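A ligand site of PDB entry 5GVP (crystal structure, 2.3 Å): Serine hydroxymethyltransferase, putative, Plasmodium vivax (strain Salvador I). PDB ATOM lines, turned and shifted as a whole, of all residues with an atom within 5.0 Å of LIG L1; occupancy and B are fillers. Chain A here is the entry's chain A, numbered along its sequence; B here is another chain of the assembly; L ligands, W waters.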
ATOM      1  N   ILE A  32       1.949 -14.461  27.559  1.00  0.00           N
ATOM      2  CA  ILE A  32       1.322 -15.482  26.704  1.00  0.00           C
ATOM      3  C   ILE A  32       1.823 -15.217  25.289  1.00  0.00           C
ATOM      4  O   ILE A  32       1.675 -14.141  24.793  1.00  0.00           O
ATOM      5  CB  ILE A  32      -0.219 -15.463  26.734  1.00  0.00           C
ATOM      6  CG1 ILE A  32      -0.765 -15.697  28.158  1.00  0.00           C
ATOM      7  CG2 ILE A  32      -0.768 -16.499  25.793  1.00  0.00           C
ATOM      8  CD1 ILE A  32      -0.668 -17.135  28.644  1.00  0.00           C
ATOM      9  N   SER A  34       0.963 -16.115  22.439  1.00  0.00           N
ATOM     10  CA  SER A  34      -0.119 -15.842  21.512  1.00  0.00           C
ATOM     11  C   SER A  34      -0.957 -14.585  21.768  1.00  0.00           C
ATOM     12  O   SER A  34      -1.850 -14.326  20.984  1.00  0.00           O
ATOM     13  CB  SER A  34      -1.049 -17.034  21.451  1.00  0.00           C
ATOM     14  OG  SER A  34      -1.470 -17.370  22.759  1.00  0.00           O
ATOM     15  N   SER A 100     -11.510 -17.390  12.474  1.00  0.00           N
ATOM     16  CA  SER A 100     -10.405 -17.594  13.418  1.00  0.00           C
ATOM     17  C   SER A 100      -9.384 -18.574  12.814  1.00  0.00           C
ATOM     18  O   SER A 100      -9.660 -19.229  11.802  1.00  0.00           O
ATOM     19  CB  SER A 100     -10.936 -18.196  14.728  1.00  0.00           C
ATOM     20  OG  SER A 100     -10.375 -17.580  15.906  1.00  0.00           O
ATOM     21  N   GLY A 101      -8.248 -18.710  13.471  1.00  0.00           N
ATOM     22  CA  GLY A 101      -7.182 -19.573  13.025  1.00  0.00           C
ATOM     23  C   GLY A 101      -7.524 -21.028  12.738  1.00  0.00           C
ATOM     24  O   GLY A 101      -7.097 -21.588  11.721  1.00  0.00           O
ATOM     25  N   SER A 102      -8.280 -21.646  13.643  1.00  0.00           N
ATOM     26  CA  SER A 102      -8.627 -23.058  13.509  1.00  0.00           C
ATOM     27  C   SER A 102      -9.571 -23.239  12.306  1.00  0.00           C
ATOM     28  O   SER A 102      -9.432 -24.192  11.544  1.00  0.00           O
ATOM     29  CB  SER A 102      -9.248 -23.625  14.809  1.00  0.00           C
ATOM     30  OG  SER A 102      -8.502 -23.279  15.986  1.00  0.00           O
ATOM     31  N   ALA A 103     -10.538 -22.325  12.144  1.00  0.00           N
ATOM     32  CA  ALA A 103     -11.451 -22.389  11.005  1.00  0.00           C
ATOM     33  C   ALA A 103     -10.660 -22.302   9.655  1.00  0.00           C
ATOM     34  O   ALA A 103     -10.779 -23.175   8.828  1.00  0.00           O
ATOM     35  CB  ALA A 103     -12.517 -21.297  11.105  1.00  0.00           C
ATOM     36  N   ASN A 105      -7.550 -23.046   9.064  1.00  0.00           N
ATOM     37  CA  ASN A 105      -6.809 -24.270   8.841  1.00  0.00           C
ATOM     38  C   ASN A 105      -7.692 -25.437   8.365  1.00  0.00           C
ATOM     39  O   ASN A 105      -7.311 -26.142   7.416  1.00  0.00           O
ATOM     40  CB  ASN A 105      -5.998 -24.676  10.083  1.00  0.00           C
ATOM     41  CG  ASN A 105      -4.797 -23.752  10.331  1.00  0.00           C
ATOM     42  OD1 ASN A 105      -4.392 -22.960   9.479  1.00  0.00           O
ATOM     43  ND2 ASN A 105      -4.206 -23.903  11.498  1.00  0.00           N
ATOM     44  N   HIS A 129       0.047 -27.304  16.227  1.00  0.00           N
ATOM     45  CA  HIS A 129      -1.318 -26.988  16.626  1.00  0.00           C
ATOM     46  C   HIS A 129      -2.250 -28.197  16.589  1.00  0.00           C
ATOM     47  O   HIS A 129      -1.995 -29.206  15.951  1.00  0.00           O
ATOM     48  CB  HIS A 129      -1.881 -25.836  15.763  1.00  0.00           C
ATOM     49  CG  HIS A 129      -3.048 -25.133  16.400  1.00  0.00           C
ATOM     50  ND1 HIS A 129      -4.295 -25.127  15.837  1.00  0.00           N
ATOM     51  CD2 HIS A 129      -3.164 -24.455  17.569  1.00  0.00           C
ATOM     52  CE1 HIS A 129      -5.138 -24.473  16.624  1.00  0.00           C
ATOM     53  NE2 HIS A 129      -4.462 -24.048  17.680  1.00  0.00           N
ATOM     54  N   THR A 131      -5.159 -28.145  15.137  1.00  0.00           N
ATOM     55  CA  THR A 131      -5.577 -28.197  13.709  1.00  0.00           C
ATOM     56  C   THR A 131      -4.536 -28.702  12.705  1.00  0.00           C
ATOM     57  O   THR A 131      -4.796 -28.648  11.504  1.00  0.00           O
ATOM     58  CB  THR A 131      -6.058 -26.813  13.212  1.00  0.00           C
ATOM     59  OG1 THR A 131      -5.030 -25.837  13.392  1.00  0.00           O
ATOM     60  CG2 THR A 131      -7.315 -26.404  13.975  1.00  0.00           C
ATOM     61  N   HIS A 132      -3.386 -29.206  13.171  1.00  0.00           N
ATOM     62  CA  HIS A 132      -2.430 -29.870  12.321  1.00  0.00           C
ATOM     63  C   HIS A 132      -2.561 -31.393  12.341  1.00  0.00           C
ATOM     64  O   HIS A 132      -1.654 -32.105  11.953  1.00  0.00           O
ATOM     65  CB  HIS A 132      -0.995 -29.404  12.683  1.00  0.00           C
ATOM     66  CG  HIS A 132      -0.806 -27.927  12.565  1.00  0.00           C
ATOM     67  ND1 HIS A 132       0.342 -27.288  12.984  1.00  0.00           N
ATOM     68  CD2 HIS A 132      -1.613 -26.955  12.070  1.00  0.00           C
ATOM     69  CE1 HIS A 132       0.229 -25.996  12.752  1.00  0.00           C
ATOM     70  NE2 HIS A 132      -0.943 -25.766  12.204  1.00  0.00           N
ATOM     71  N   GLY A 181       5.133 -24.854  10.466  1.00  0.00           N
ATOM     72  CA  GLY A 181       4.745 -23.613  11.200  1.00  0.00           C
ATOM     73  C   GLY A 181       3.875 -23.995  12.394  1.00  0.00           C
ATOM     74  O   GLY A 181       2.902 -24.704  12.213  1.00  0.00           O
ATOM     75  N   TYR A 182       4.245 -23.554  13.610  1.00  0.00           N
ATOM     76  CA  TYR A 182       3.770 -24.239  14.840  1.00  0.00           C
ATOM     77  C   TYR A 182       3.279 -23.305  15.960  1.00  0.00           C
ATOM     78  O   TYR A 182       3.289 -22.087  15.803  1.00  0.00           O
ATOM     79  CB  TYR A 182       4.883 -25.162  15.347  1.00  0.00           C
ATOM     80  CG  TYR A 182       5.620 -25.920  14.265  1.00  0.00           C
ATOM     81  CD1 TYR A 182       5.028 -27.018  13.638  1.00  0.00           C
ATOM     82  CD2 TYR A 182       6.891 -25.533  13.855  1.00  0.00           C
ATOM     83  CE1 TYR A 182       5.694 -27.721  12.637  1.00  0.00           C
ATOM     84  CE2 TYR A 182       7.566 -26.237  12.858  1.00  0.00           C
ATOM     85  CZ  TYR A 182       6.971 -27.340  12.263  1.00  0.00           C
ATOM     86  OH  TYR A 182       7.625 -28.030  11.266  1.00  0.00           O
ATOM     87  N   THR A 183       2.833 -23.877  17.078  1.00  0.00           N
ATOM     88  CA  THR A 183       2.286 -23.068  18.191  1.00  0.00           C
ATOM     89  C   THR A 183       3.330 -22.751  19.252  1.00  0.00           C
ATOM     90  O   THR A 183       3.366 -21.624  19.728  1.00  0.00           O
ATOM     91  CB  THR A 183       0.980 -23.599  18.849  1.00  0.00           C
ATOM     92  OG1 THR A 183       1.197 -24.088  20.180  1.00  0.00           O
ATOM     93  CG2 THR A 183       0.320 -24.631  18.016  1.00  0.00           C
ATOM     94  N   ASP A 208       1.699 -22.628   8.386  1.00  0.00           N
ATOM     95  CA  ASP A 208       0.814 -21.890   9.347  1.00  0.00           C
ATOM     96  C   ASP A 208       1.752 -20.995  10.078  1.00  0.00           C
ATOM     97  O   ASP A 208       2.500 -21.478  10.906  1.00  0.00           O
ATOM     98  CB  ASP A 208       0.124 -22.850  10.308  1.00  0.00           C
ATOM     99  CG  ASP A 208      -0.819 -22.146  11.319  1.00  0.00           C
ATOM    100  OD1 ASP A 208      -0.779 -20.927  11.581  1.00  0.00           O
ATOM    101  OD2 ASP A 208      -1.656 -22.881  11.867  1.00  0.00           O
ATOM    102  N   SER A 210       0.940 -18.245  12.023  1.00  0.00           N
ATOM    103  CA  SER A 210       0.199 -17.464  13.043  1.00  0.00           C
ATOM    104  C   SER A 210       1.048 -16.869  14.154  1.00  0.00           C
ATOM    105  O   SER A 210       0.919 -15.693  14.467  1.00  0.00           O
ATOM    106  CB  SER A 210      -0.889 -18.317  13.659  1.00  0.00           C
ATOM    107  OG  SER A 210      -1.859 -18.607  12.665  1.00  0.00           O
ATOM    108  N   HIS A 211       1.935 -17.682  14.712  1.00  0.00           N
ATOM    109  CA  HIS A 211       2.885 -17.200  15.733  1.00  0.00           C
ATOM    110  C   HIS A 211       4.026 -16.326  15.256  1.00  0.00           C
ATOM    111  O   HIS A 211       4.571 -15.555  16.054  1.00  0.00           O
ATOM    112  CB  HIS A 211       3.464 -18.364  16.529  1.00  0.00           C
ATOM    113  CG  HIS A 211       2.637 -18.704  17.710  1.00  0.00           C
ATOM    114  ND1 HIS A 211       2.602 -17.923  18.846  1.00  0.00           N
ATOM    115  CD2 HIS A 211       1.747 -19.703  17.919  1.00  0.00           C
ATOM    116  CE1 HIS A 211       1.765 -18.450  19.712  1.00  0.00           C
ATOM    117  NE2 HIS A 211       1.238 -19.527  19.171  1.00  0.00           N
ATOM    118  N   THR A 234      -3.365 -16.329  11.725  1.00  0.00           N
ATOM    119  CA  THR A 234      -4.272 -15.516  12.530  1.00  0.00           C
ATOM    120  C   THR A 234      -3.818 -14.079  12.471  1.00  0.00           C
ATOM    121  O   THR A 234      -2.673 -13.824  12.191  1.00  0.00           O
ATOM    122  CB  THR A 234      -4.285 -15.986  13.996  1.00  0.00           C
ATOM    123  OG1 THR A 234      -2.959 -15.937  14.545  1.00  0.00           O
ATOM    124  CG2 THR A 234      -4.814 -17.396  14.085  1.00  0.00           C
ATOM    125  N   HIS A 236      -4.431 -11.945  15.261  1.00  0.00           N
ATOM    126  CA  HIS A 236      -4.528 -11.454  16.665  1.00  0.00           C
ATOM    127  C   HIS A 236      -3.293 -11.628  17.544  1.00  0.00           C
ATOM    128  O   HIS A 236      -3.237 -11.038  18.615  1.00  0.00           O
ATOM    129  CB  HIS A 236      -5.729 -12.041  17.420  1.00  0.00           C
ATOM    130  CG  HIS A 236      -5.933 -13.511  17.213  1.00  0.00           C
ATOM    131  ND1 HIS A 236      -6.525 -14.021  16.088  1.00  0.00           N
ATOM    132  CD2 HIS A 236      -5.658 -14.568  18.008  1.00  0.00           C
ATOM    133  CE1 HIS A 236      -6.614 -15.334  16.200  1.00  0.00           C
ATOM    134  NE2 HIS A 236      -6.087 -15.690  17.352  1.00  0.00           N
ATOM    135  N   LYS A 237      -2.335 -12.439  17.110  1.00  0.00           N
ATOM    136  CA  LYS A 237      -1.134 -12.662  17.899  1.00  0.00           C
ATOM    137  C   LYS A 237      -0.114 -11.549  17.650  1.00  0.00           C
ATOM    138  O   LYS A 237      -0.425 -10.362  17.878  1.00  0.00           O
ATOM    139  CB  LYS A 237      -0.596 -14.051  17.618  1.00  0.00           C
ATOM    140  CG  LYS A 237      -1.593 -15.154  17.895  1.00  0.00           C
ATOM    141  CD  LYS A 237      -0.965 -16.484  17.572  1.00  0.00           C
ATOM    142  CE  LYS A 237      -1.931 -17.599  17.798  1.00  0.00           C
ATOM    143  NZ  LYS A 237      -3.149 -17.479  16.992  1.00  0.00           N
ATOM    144  N   ARG A 243      -9.188 -10.617  16.400  1.00  0.00           N
ATOM    145  CA  ARG A 243      -9.279 -12.068  16.322  1.00  0.00           C
ATOM    146  C   ARG A 243      -9.878 -12.439  14.944  1.00  0.00           C
ATOM    147  O   ARG A 243     -11.066 -12.290  14.748  1.00  0.00           O
ATOM    148  CB  ARG A 243     -10.114 -12.657  17.475  1.00  0.00           C
ATOM    149  CG  ARG A 243      -9.667 -12.177  18.856  1.00  0.00           C
ATOM    150  CD  ARG A 243     -10.325 -12.975  19.993  1.00  0.00           C
ATOM    151  NE  ARG A 243      -9.647 -14.255  20.161  1.00  0.00           N
ATOM    152  CZ  ARG A 243      -8.541 -14.451  20.873  1.00  0.00           C
ATOM    153  NH1 ARG A 243      -7.933 -13.457  21.507  1.00  0.00           N
ATOM    154  NH2 ARG A 243      -8.027 -15.659  20.907  1.00  0.00           N
ATOM    155  N   ARG A 371       5.703 -21.961  28.452  1.00  0.00           N
ATOM    156  CA  ARG A 371       6.003 -21.213  27.294  1.00  0.00           C
ATOM    157  C   ARG A 371       5.745 -19.771  27.652  1.00  0.00           C
ATOM    158  O   ARG A 371       4.757 -19.470  28.369  1.00  0.00           O
ATOM    159  CB  ARG A 371       5.119 -21.694  26.145  1.00  0.00           C
ATOM    160  CG  ARG A 371       5.261 -20.937  24.845  1.00  0.00           C
ATOM    161  CD  ARG A 371       4.128 -21.253  23.891  1.00  0.00           C
ATOM    162  NE  ARG A 371       2.882 -20.600  24.288  1.00  0.00           N
ATOM    163  CZ  ARG A 371       1.829 -20.436  23.494  1.00  0.00           C
ATOM    164  NH1 ARG A 371       1.844 -20.873  22.222  1.00  0.00           N
ATOM    165  NH2 ARG A 371       0.749 -19.794  23.959  1.00  0.00           N
ATOM    166  N   TYR B  54      -6.784 -14.910  25.465  1.00  0.00           N
ATOM    167  CA  TYR B  54      -6.892 -16.335  25.045  1.00  0.00           C
ATOM    168  C   TYR B  54      -7.463 -17.209  26.188  1.00  0.00           C
ATOM    169  O   TYR B  54      -6.889 -17.277  27.265  1.00  0.00           O
ATOM    170  CB  TYR B  54      -5.526 -16.908  24.569  1.00  0.00           C
ATOM    171  CG  TYR B  54      -5.500 -17.302  23.105  1.00  0.00           C
ATOM    172  CD1 TYR B  54      -6.168 -18.452  22.668  1.00  0.00           C
ATOM    173  CD2 TYR B  54      -4.809 -16.534  22.164  1.00  0.00           C
ATOM    174  CE1 TYR B  54      -6.159 -18.804  21.331  1.00  0.00           C
ATOM    175  CE2 TYR B  54      -4.795 -16.900  20.810  1.00  0.00           C
ATOM    176  CZ  TYR B  54      -5.482 -18.022  20.402  1.00  0.00           C
ATOM    177  OH  TYR B  54      -5.475 -18.363  19.074  1.00  0.00           O
ATOM    178  N   GLU B  56      -8.924 -20.796  25.854  1.00  0.00           N
ATOM    179  CA  GLU B  56      -9.303 -22.109  25.358  1.00  0.00           C
ATOM    180  C   GLU B  56      -9.770 -23.063  26.439  1.00  0.00           C
ATOM    181  O   GLU B  56      -9.115 -23.215  27.456  1.00  0.00           O
ATOM    182  CB  GLU B  56      -8.127 -22.771  24.661  1.00  0.00           C
ATOM    183  CG  GLU B  56      -7.713 -22.115  23.359  1.00  0.00           C
ATOM    184  CD  GLU B  56      -6.436 -22.710  22.830  1.00  0.00           C
ATOM    185  OE1 GLU B  56      -5.364 -22.260  23.270  1.00  0.00           O
ATOM    186  OE2 GLU B  56      -6.488 -23.654  22.034  1.00  0.00           O
ATOM    187  N   TYR B  64      -5.397 -21.882  30.187  1.00  0.00           N
ATOM    188  CA  TYR B  64      -4.633 -20.844  30.906  1.00  0.00           C
ATOM    189  C   TYR B  64      -5.348 -20.327  32.124  1.00  0.00           C
ATOM    190  O   TYR B  64      -6.550 -20.507  32.277  1.00  0.00           O
ATOM    191  CB  TYR B  64      -4.323 -19.651  30.008  1.00  0.00           C
ATOM    192  CG  TYR B  64      -3.805 -20.007  28.655  1.00  0.00           C
ATOM    193  CD1 TYR B  64      -3.171 -21.243  28.424  1.00  0.00           C
ATOM    194  CD2 TYR B  64      -3.918 -19.117  27.609  1.00  0.00           C
ATOM    195  CE1 TYR B  64      -2.698 -21.557  27.165  1.00  0.00           C
ATOM    196  CE2 TYR B  64      -3.445 -19.431  26.350  1.00  0.00           C
ATOM    197  CZ  TYR B  64      -2.833 -20.641  26.127  1.00  0.00           C
ATOM    198  OH  TYR B  64      -2.376 -20.950  24.882  1.00  0.00           O
ATOM    199  N   GLN B 270     -13.064 -25.483  17.000  1.00  0.00           N
ATOM    200  CA  GLN B 270     -12.518 -24.172  17.333  1.00  0.00           C
ATOM    201  C   GLN B 270     -11.298 -24.268  18.244  1.00  0.00           C
ATOM    202  O   GLN B 270     -10.953 -25.360  18.734  1.00  0.00           O
ATOM    203  CB  GLN B 270     -13.609 -23.259  17.955  1.00  0.00           C
ATOM    204  CG  GLN B 270     -14.816 -23.116  17.028  1.00  0.00           C
ATOM    205  CD  GLN B 270     -15.867 -22.080  17.410  1.00  0.00           C
ATOM    206  OE1 GLN B 270     -16.780 -21.807  16.627  1.00  0.00           O
ATOM    207  NE2 GLN B 270     -15.780 -21.540  18.602  1.00  0.00           N
ATOM    208  N   GLY B 271     -10.648 -23.121  18.412  1.00  0.00           N
ATOM    209  CA  GLY B 271      -9.621 -22.893  19.408  1.00  0.00           C
ATOM    210  C   GLY B 271     -10.142 -21.866  20.420  1.00  0.00           C
ATOM    211  O   GLY B 271     -11.168 -22.072  21.054  1.00  0.00           O
ATOM    212  N   GLY B 272      -9.454 -20.736  20.519  1.00  0.00           N
ATOM    213  CA  GLY B 272      -9.823 -19.678  21.442  1.00  0.00           C
ATOM    214  C   GLY B 272     -11.176 -19.035  21.184  1.00  0.00           C
ATOM    215  O   GLY B 272     -11.464 -18.649  20.044  1.00  0.00           O
HETATM  216  N1  LIG L   1      -2.554 -21.998  14.295  1.00  0.00           N
HETATM  217  C1  LIG L   1      -1.529 -21.901  15.154  1.00  0.00           C
HETATM  218  C2  LIG L   1      -0.127 -22.201  14.700  1.00  0.00           C
HETATM  219  C3  LIG L   1      -1.819 -21.488  16.552  1.00  0.00           C
HETATM  220  O1  LIG L   1      -0.830 -21.380  17.449  1.00  0.00           O
HETATM  221  C4  LIG L   1      -3.210 -21.209  16.949  1.00  0.00           C
HETATM  222  C5  LIG L   1      -3.533 -20.786  18.376  1.00  0.00           C
HETATM  223  C6  LIG L   1      -4.236 -21.357  15.870  1.00  0.00           C
HETATM  224  C7  LIG L   1      -3.825 -21.774  14.598  1.00  0.00           C
HETATM  225  C8  LIG L   1      -5.720 -21.169  16.074  1.00  0.00           C
HETATM  226  O2  LIG L   1      -6.146 -19.841  16.280  1.00  0.00           O
HETATM  227  P1  LIG L   1      -7.635 -19.581  16.851  1.00  0.00           P
HETATM  228  O3  LIG L   1      -8.516 -20.675  16.316  1.00  0.00           O
HETATM  229  O4  LIG L   1      -7.459 -19.714  18.331  1.00  0.00           O
HETATM  230  O5  LIG L   1      -7.826 -18.159  16.428  1.00  0.00           O
HETATM  231  C9  LIG L   1      -1.686 -20.364  21.466  1.00  0.00           C
HETATM  232  O6  LIG L   1      -1.822 -19.770  22.526  1.00  0.00           O
HETATM  233  O7  LIG L   1      -0.565 -20.437  20.941  1.00  0.00           O
HETATM  234  C10 LIG L   1      -2.910 -20.990  20.817  1.00  0.00           C
HETATM  235  N2  LIG L   1      -2.716 -21.363  19.427  1.00  0.00           N
HETATM  236  O1  LG2 L   2      -6.204 -34.140  28.358  1.00  0.00           O
HETATM  237  C1  LG2 L   2      -6.399 -34.227  27.115  1.00  0.00           C
HETATM  238  O2  LG2 L   2      -7.511 -34.564  26.623  1.00  0.00           O
HETATM  239  C2  LG2 L   2      -5.222 -33.912  26.210  1.00  0.00           C
HETATM  240  C3  LG2 L   2      -5.600 -33.447  24.787  1.00  0.00           C
HETATM  241  C4  LG2 L   2      -5.609 -31.941  24.683  1.00  0.00           C
HETATM  242  C5  LG2 L   2      -4.457 -31.238  24.981  1.00  0.00           C
HETATM  243  C6  LG2 L   2      -6.753 -31.276  24.273  1.00  0.00           C
HETATM  244  C7  LG2 L   2      -6.745 -29.896  24.169  1.00  0.00           C
HETATM  245  C8  LG2 L   2      -5.588 -29.192  24.480  1.00  0.00           C
HETATM  246  C9  LG2 L   2      -4.441 -29.859  24.880  1.00  0.00           C
HETATM  247  C10 LG2 L   2      -3.219 -29.092  25.214  1.00  0.00           C
HETATM  248  C11 LG2 L   2      -2.534 -29.394  26.373  1.00  0.00           C
HETATM  249  C12 LG2 L   2      -1.398 -28.672  26.715  1.00  0.00           C
HETATM  250  C13 LG2 L   2      -0.653 -29.008  28.005  1.00  0.00           C
HETATM  251  F1  LG2 L   2       0.435 -28.283  28.228  1.00  0.00           F
HETATM  252  F2  LG2 L   2      -1.467 -28.879  29.035  1.00  0.00           F
HETATM  253  F3  LG2 L   2      -0.300 -30.283  27.933  1.00  0.00           F
HETATM  254  C14 LG2 L   2      -0.943 -27.650  25.889  1.00  0.00           C
HETATM  255  C15 LG2 L   2      -2.764 -28.084  24.358  1.00  0.00           C
HETATM  256  C16 LG2 L   2      -1.625 -27.314  24.680  1.00  0.00           C
HETATM  257  C17 LG2 L   2      -1.108 -26.225  23.754  1.00  0.00           C
HETATM  258  C18 LG2 L   2      -0.519 -24.979  24.481  1.00  0.00           C
HETATM  259  C19 LG2 L   2      -0.050 -23.851  23.550  1.00  0.00           C
HETATM  260  C20 LG2 L   2      -1.437 -24.362  25.564  1.00  0.00           C
HETATM  261  C21 LG2 L   2       0.051 -26.846  22.954  1.00  0.00           C
HETATM  262  C22 LG2 L   2       0.963 -27.422  23.626  1.00  0.00           C
HETATM  263  N1  LG2 L   2       1.792 -27.959  24.245  1.00  0.00           N
HETATM  264  C23 LG2 L   2       0.155 -26.746  21.603  1.00  0.00           C
HETATM  265  N2  LG2 L   2       1.151 -27.244  20.887  1.00  0.00           N
HETATM  266  C24 LG2 L   2      -2.187 -25.746  22.829  1.00  0.00           C
HETATM  267  C25 LG2 L   2      -3.579 -25.240  23.012  1.00  0.00           C
HETATM  268  C26 LG2 L   2      -4.357 -25.043  24.284  1.00  0.00           C
HETATM  269  N3  LG2 L   2      -4.038 -24.991  21.768  1.00  0.00           N
HETATM  270  N4  LG2 L   2      -3.119 -25.285  20.726  1.00  0.00           N
HETATM  271  C27 LG2 L   2      -2.037 -25.710  21.378  1.00  0.00           C
HETATM  272  O3  LG2 L   2      -0.860 -26.097  20.809  1.00  0.00           O
HETATM  273  O   HOH W   1     -11.200 -20.212  17.289  1.00  0.00           O
HETATM  274  O   HOH W   2      -6.051 -22.450  19.472  1.00  0.00           O
HETATM  275  O   HOH W   3      -9.042 -16.859  18.849  1.00  0.00           O
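The guanidinium group (NH2) of Arg 371 lies within hydrogen-bond range of the side-chain hydroxyl (OG) of Ser 34 (3.5 Å). The side-chain hydroxyl of Tyr 54 of chain B is in hydrogen-bond range of a ring nitrogen (NE2) of His 236 (3.2 Å). OH of Tyr 54 of chain B lies within hydrogen-bond range of NZ of Lys 237 (3.2 Å). NE2 of His 211 sits at hydrogen-bond distance from O of Thr 183 (3.0 Å). OH of Tyr 64 of chain B is in hydrogen-bond range of NH2 of Arg 371, at 3.5 Å. OG of Ser 210 is in hydrogen-bond range of OD1 of Asp 208 (2.8 Å). NH1 of Arg 371 sits at hydrogen-bond distance from O of Thr 183 (3.0 Å). The side-chain hydroxyl (OG1) of Thr 131 is in hydrogen-bond range of the side-chain amide nitrogen (ND2) of Asn 105.
Residues that only touch LIG L1: Thr 183 (3.2 Å), His 129 (3.2 Å), Thr 234 (3.5 Å), Tyr 182 (3.6 Å), Lys 237 (3.6 Å), Glu 56 of chain B (3.7 Å), Asn 105 (3.8 Å), Ser 210 (3.8 Å) and Gly 271 of chain B (3.9 Å). Hydrophobic or aromatic side chains within 4 Å of LIG L1: His 129, His 211, His 236, Tyr 54 of chain B and Tyr 64 of chain B.
Water W1 lies within hydrogen-bond range of O3 of LIG L1, OG of Ser 100, N of Gly 271 of chain B and O of Gly 272 of chain B. Water W3 lies within hydrogen-bond range of the guanidinium group of Arg 243, an oxygen (O5) of LIG L1, the backbone carbonyl oxygen of Gly 272 of chain B and the side-chain hydroxyl of Ser 100. Water W2 lies within hydrogen-bond range of the side-chain carboxylate of Glu 56 of chain B (2.9 Å), a ring nitrogen (NE2) of His 129 (2.9 Å) and an oxygen (O4) of LIG L1 (3.3 Å).
The side-chain hydroxyl (OG) of Ser 34 sits at hydrogen-bond distance from an oxygen (O6) of LIG L1 (2.4 Å). The side-chain hydroxyl (OH) of Tyr 54 of chain B lies within hydrogen-bond range of an oxygen (O4) of LIG L1 (2.5 Å). An oxygen (O3) of LIG L1 lies within hydrogen-bond range of the backbone NH (N) of Ser 102 (2.9 Å). An oxygen (O3) of LIG L1 lies within hydrogen-bond range of the side-chain hydroxyl (OG) of Ser 102 (2.6 Å). O5 of LIG L1 is in hydrogen-bond range of OG of Ser 100 (2.7 Å). A ring nitrogen (NE2) of His 211 lies within hydrogen-bond range of an oxygen (O7) of LIG L1. OH of Tyr 64 of chain B is in hydrogen-bond range of O6 of LIG L1 (2.7 Å). The side-chain carboxylate (OD2) of Asp 208 is in hydrogen-bond range of a nitrogen (N1) of LIG L1 (2.7 Å). An oxygen (O7) of LIG L1 lies within salt-bridge range of the guanidinium group of Arg 371 (2.8 Å). An oxygen (O5) of LIG L1 is in hydrogen-bond range of the backbone NH (N) of Gly 101 (3.0 Å). O5 of LIG L1 lies close to NE2 of His 236. An oxygen (O4) of LIG L1 sits at hydrogen-bond distance from the backbone NH (N) of Gly 272 of chain B. OG1 of Thr 183 lies within hydrogen-bond range of O3 of LG2 L2. The side-chain carboxylate of Glu 56 of chain B sits at hydrogen-bond distance from a nitrogen (N3) of LG2 L2 (2.8 Å).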
